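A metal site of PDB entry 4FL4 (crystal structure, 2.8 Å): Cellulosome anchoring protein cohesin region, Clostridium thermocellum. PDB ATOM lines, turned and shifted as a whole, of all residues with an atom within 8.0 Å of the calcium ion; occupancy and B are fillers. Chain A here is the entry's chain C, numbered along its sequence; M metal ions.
The calcium ion is bound by OD1 of Asp 262 (2.5 Å), OD1 of Asp 251 (2.5 Å), OD2 of Asp 262 (2.5 Å), O of Ser 257 (2.6 Å), O of Val 253 (2.6 Å) and OD2 of Asp 255 (2.7 Å).
The side-chain carboxylate of Asp 251 is in salt-bridge range of the side-chain amino group of Lys 254 (3.8 Å). The backbone NH (N) of Asp 251 sits at hydrogen-bond distance from the backbone carbonyl oxygen (O) of Thr 221 (2.9 Å). The backbone NH (N) of Asn 259 sits close to the side-chain carboxylate (OD2) of Asp 262. OD1 of Asp 262 lies close to N of Ile 252 (2.6 Å). The backbone NH (N) of Asn 256 lies within hydrogen-bond range of the side-chain carboxylate (OD2) of Asp 251 (3.0 Å).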
ATOM      1  N   THR A 221      16.163  21.413 -32.008  1.00  0.00           N
ATOM      2  CA  THR A 221      16.274  21.588 -30.558  1.00  0.00           C
ATOM      3  C   THR A 221      16.673  22.997 -30.203  1.00  0.00           C
ATOM      4  O   THR A 221      16.718  23.376 -29.030  1.00  0.00           O
ATOM      5  CB  THR A 221      17.256  20.596 -29.859  1.00  0.00           C
ATOM      6  OG1 THR A 221      18.622  21.012 -30.013  1.00  0.00           O
ATOM      7  CG2 THR A 221      17.077  19.154 -30.365  1.00  0.00           C
ATOM      8  N   TYR A 222      16.955  23.790 -31.229  1.00  0.00           N
ATOM      9  CA  TYR A 222      17.384  25.163 -30.982  1.00  0.00           C
ATOM     10  C   TYR A 222      16.301  26.204 -31.273  1.00  0.00           C
ATOM     11  O   TYR A 222      15.447  26.024 -32.150  1.00  0.00           O
ATOM     12  CB  TYR A 222      18.637  25.474 -31.769  1.00  0.00           C
ATOM     13  CG  TYR A 222      19.902  24.911 -31.162  1.00  0.00           C
ATOM     14  CD1 TYR A 222      20.633  25.640 -30.210  1.00  0.00           C
ATOM     15  CD2 TYR A 222      20.363  23.650 -31.540  1.00  0.00           C
ATOM     16  CE1 TYR A 222      21.801  25.126 -29.666  1.00  0.00           C
ATOM     17  CE2 TYR A 222      21.520  23.128 -31.000  1.00  0.00           C
ATOM     18  CZ  TYR A 222      22.234  23.870 -30.068  1.00  0.00           C
ATOM     19  OH  TYR A 222      23.387  23.325 -29.549  1.00  0.00           O
ATOM     20  N   LEU A 223      16.355  27.284 -30.499  1.00  0.00           N
ATOM     21  CA  LEU A 223      15.500  28.440 -30.725  1.00  0.00           C
ATOM     22  C   LEU A 223      15.990  29.223 -31.950  1.00  0.00           C
ATOM     23  O   LEU A 223      17.044  29.867 -31.899  1.00  0.00           O
ATOM     24  CB  LEU A 223      15.530  29.341 -29.493  1.00  0.00           C
ATOM     25  CG  LEU A 223      14.405  30.378 -29.507  1.00  0.00           C
ATOM     26  CD1 LEU A 223      13.064  29.668 -29.503  1.00  0.00           C
ATOM     27  CD2 LEU A 223      14.512  31.363 -28.347  1.00  0.00           C
ATOM     28  N   GLY A 250      16.996  24.304 -26.452  1.00  0.00           N
ATOM     29  CA  GLY A 250      15.822  24.021 -25.663  1.00  0.00           C
ATOM     30  C   GLY A 250      14.501  24.331 -26.329  1.00  0.00           C
ATOM     31  O   GLY A 250      13.467  24.345 -25.666  1.00  0.00           O
ATOM     32  N   ASP A 251      14.495  24.604 -27.630  1.00  0.00           N
ATOM     33  CA  ASP A 251      13.210  24.666 -28.305  1.00  0.00           C
ATOM     34  C   ASP A 251      12.910  23.299 -28.900  1.00  0.00           C
ATOM     35  O   ASP A 251      12.941  23.138 -30.122  1.00  0.00           O
ATOM     36  CB  ASP A 251      13.180  25.737 -29.389  1.00  0.00           C
ATOM     37  CG  ASP A 251      11.779  25.968 -29.916  1.00  0.00           C
ATOM     38  OD1 ASP A 251      10.837  25.494 -29.253  1.00  0.00           O
ATOM     39  OD2 ASP A 251      11.608  26.619 -30.968  1.00  0.00           O
ATOM     40  N   ILE A 252      12.646  22.309 -28.039  1.00  0.00           N
ATOM     41  CA  ILE A 252      12.517  20.928 -28.479  1.00  0.00           C
ATOM     42  C   ILE A 252      11.185  20.654 -29.181  1.00  0.00           C
ATOM     43  O   ILE A 252      11.140  19.863 -30.129  1.00  0.00           O
ATOM     44  CB  ILE A 252      12.732  19.869 -27.358  1.00  0.00           C
ATOM     45  CG1 ILE A 252      14.158  19.882 -26.814  1.00  0.00           C
ATOM     46  CG2 ILE A 252      12.472  18.463 -27.907  1.00  0.00           C
ATOM     47  CD1 ILE A 252      14.568  21.154 -26.207  1.00  0.00           C
ATOM     48  N   VAL A 253      10.103  21.277 -28.713  1.00  0.00           N
ATOM     49  CA  VAL A 253       8.885  21.198 -29.500  1.00  0.00           C
ATOM     50  C   VAL A 253       8.748  22.528 -30.244  1.00  0.00           C
ATOM     51  O   VAL A 253       8.294  23.525 -29.701  1.00  0.00           O
ATOM     52  CB  VAL A 253       7.614  20.732 -28.682  1.00  0.00           C
ATOM     53  CG1 VAL A 253       8.027  19.821 -27.532  1.00  0.00           C
ATOM     54  CG2 VAL A 253       6.788  21.885 -28.171  1.00  0.00           C
ATOM     55  N   LYS A 254       9.212  22.539 -31.497  1.00  0.00           N
ATOM     56  CA  LYS A 254       9.403  23.778 -32.234  1.00  0.00           C
ATOM     57  C   LYS A 254       8.166  24.655 -32.213  1.00  0.00           C
ATOM     58  O   LYS A 254       7.143  24.321 -32.821  1.00  0.00           O
ATOM     59  CB  LYS A 254       9.846  23.508 -33.672  1.00  0.00           C
ATOM     60  CG  LYS A 254      11.356  23.344 -33.867  1.00  0.00           C
ATOM     61  CD  LYS A 254      12.041  24.698 -34.089  1.00  0.00           C
ATOM     62  CE  LYS A 254      11.324  25.520 -35.152  1.00  0.00           C
ATOM     63  NZ  LYS A 254      11.099  26.941 -34.690  1.00  0.00           N
ATOM     64  N   ASP A 255       8.254  25.769 -31.507  1.00  0.00           N
ATOM     65  CA  ASP A 255       7.170  26.746 -31.430  1.00  0.00           C
ATOM     66  C   ASP A 255       7.708  28.131 -31.083  1.00  0.00           C
ATOM     67  O   ASP A 255       6.944  29.071 -30.846  1.00  0.00           O
ATOM     68  CB  ASP A 255       6.038  26.305 -30.457  1.00  0.00           C
ATOM     69  CG  ASP A 255       6.515  26.065 -29.018  1.00  0.00           C
ATOM     70  OD1 ASP A 255       5.922  25.195 -28.351  1.00  0.00           O
ATOM     71  OD2 ASP A 255       7.454  26.744 -28.545  1.00  0.00           O
ATOM     72  N   ASN A 256       9.030  28.245 -31.041  1.00  0.00           N
ATOM     73  CA  ASN A 256       9.678  29.532 -30.825  1.00  0.00           C
ATOM     74  C   ASN A 256       9.516  30.070 -29.415  1.00  0.00           C
ATOM     75  O   ASN A 256       9.579  31.286 -29.174  1.00  0.00           O
ATOM     76  CB  ASN A 256       9.180  30.558 -31.844  1.00  0.00           C
ATOM     77  CG  ASN A 256       9.811  30.371 -33.205  1.00  0.00           C
ATOM     78  OD1 ASN A 256      10.738  31.095 -33.548  1.00  0.00           O
ATOM     79  ND2 ASN A 256       9.329  29.398 -33.975  1.00  0.00           N
ATOM     80  N   SER A 257       9.281  29.141 -28.480  1.00  0.00           N
ATOM     81  CA  SER A 257       9.293  29.412 -27.052  1.00  0.00           C
ATOM     82  C   SER A 257      10.006  28.276 -26.381  1.00  0.00           C
ATOM     83  O   SER A 257       9.840  27.135 -26.794  1.00  0.00           O
ATOM     84  CB  SER A 257       7.877  29.475 -26.500  1.00  0.00           C
ATOM     85  OG  SER A 257       7.312  30.749 -26.650  1.00  0.00           O
ATOM     86  N   ILE A 258      10.801  28.597 -25.369  1.00  0.00           N
ATOM     87  CA  ILE A 258      11.396  27.587 -24.502  1.00  0.00           C
ATOM     88  C   ILE A 258      10.586  27.477 -23.195  1.00  0.00           C
ATOM     89  O   ILE A 258      10.621  28.372 -22.348  1.00  0.00           O
ATOM     90  CB  ILE A 258      12.893  27.905 -24.225  1.00  0.00           C
ATOM     91  CG1 ILE A 258      13.661  28.000 -25.556  1.00  0.00           C
ATOM     92  CG2 ILE A 258      13.519  26.867 -23.310  1.00  0.00           C
ATOM     93  CD1 ILE A 258      15.191  27.982 -25.413  1.00  0.00           C
ATOM     94  N   ASN A 259       9.817  26.397 -23.072  1.00  0.00           N
ATOM     95  CA  ASN A 259       8.903  26.235 -21.925  1.00  0.00           C
ATOM     96  C   ASN A 259       8.673  24.790 -21.456  1.00  0.00           C
ATOM     97  O   ASN A 259       9.462  23.890 -21.770  1.00  0.00           O
ATOM     98  CB  ASN A 259       7.575  26.935 -22.212  1.00  0.00           C
ATOM     99  CG  ASN A 259       6.945  26.481 -23.526  1.00  0.00           C
ATOM    100  OD1 ASN A 259       7.097  25.333 -23.942  1.00  0.00           O
ATOM    101  ND2 ASN A 259       6.253  27.400 -24.195  1.00  0.00           N
ATOM    102  N   LEU A 260       7.594  24.556 -20.695  1.00  0.00           N
ATOM    103  CA  LEU A 260       7.367  23.261 -20.065  1.00  0.00           C
ATOM    104  C   LEU A 260       7.314  22.155 -21.079  1.00  0.00           C
ATOM    105  O   LEU A 260       7.879  21.077 -20.870  1.00  0.00           O
ATOM    106  CB  LEU A 260       6.059  23.241 -19.277  1.00  0.00           C
ATOM    107  CG  LEU A 260       5.990  24.013 -17.961  1.00  0.00           C
ATOM    108  CD1 LEU A 260       4.576  23.946 -17.419  1.00  0.00           C
ATOM    109  CD2 LEU A 260       7.020  23.495 -16.948  1.00  0.00           C
ATOM    110  N   LEU A 261       6.621  22.413 -22.186  1.00  0.00           N
ATOM    111  CA  LEU A 261       6.464  21.422 -23.236  1.00  0.00           C
ATOM    112  C   LEU A 261       7.807  20.902 -23.704  1.00  0.00           C
ATOM    113  O   LEU A 261       7.926  19.754 -24.104  1.00  0.00           O
ATOM    114  CB  LEU A 261       5.723  22.024 -24.416  1.00  0.00           C
ATOM    115  CG  LEU A 261       4.274  22.354 -24.099  1.00  0.00           C
ATOM    116  CD1 LEU A 261       3.689  23.312 -25.128  1.00  0.00           C
ATOM    117  CD2 LEU A 261       3.529  21.038 -24.058  1.00  0.00           C
ATOM    118  N   ASP A 262       8.813  21.773 -23.666  1.00  0.00           N
ATOM    119  CA  ASP A 262      10.159  21.412 -24.090  1.00  0.00           C
ATOM    120  C   ASP A 262      10.868  20.539 -23.060  1.00  0.00           C
ATOM    121  O   ASP A 262      11.388  19.454 -23.387  1.00  0.00           O
ATOM    122  CB  ASP A 262      10.999  22.661 -24.373  1.00  0.00           C
ATOM    123  CG  ASP A 262      10.464  23.481 -25.538  1.00  0.00           C
ATOM    124  OD1 ASP A 262      10.524  23.026 -26.713  1.00  0.00           O
ATOM    125  OD2 ASP A 262      10.002  24.623 -25.265  1.00  0.00           O
ATOM    126  N   VAL A 263      10.901  21.021 -21.814  1.00  0.00           N
ATOM    127  CA  VAL A 263      11.525  20.292 -20.717  1.00  0.00           C
ATOM    128  C   VAL A 263      10.890  18.903 -20.589  1.00  0.00           C
ATOM    129  O   VAL A 263      11.576  17.919 -20.321  1.00  0.00           O
ATOM    130  CB  VAL A 263      11.393  21.061 -19.391  1.00  0.00           C
ATOM    131  CG1 VAL A 263      11.772  20.181 -18.245  1.00  0.00           C
ATOM    132  CG2 VAL A 263      12.267  22.316 -19.403  1.00  0.00           C
ATOM    133  N   ALA A 305      12.011  32.021 -22.837  1.00  0.00           N
ATOM    134  CA  ALA A 305      12.504  32.809 -23.950  1.00  0.00           C
ATOM    135  C   ALA A 305      11.738  32.527 -25.237  1.00  0.00           C
ATOM    136  O   ALA A 305      11.276  31.416 -25.458  1.00  0.00           O
ATOM    137  CB  ALA A 305      13.959  32.539 -24.154  1.00  0.00           C
HETATM  138 CA    CA M   1       9.036  24.829 -27.600  1.00  0.00          CA
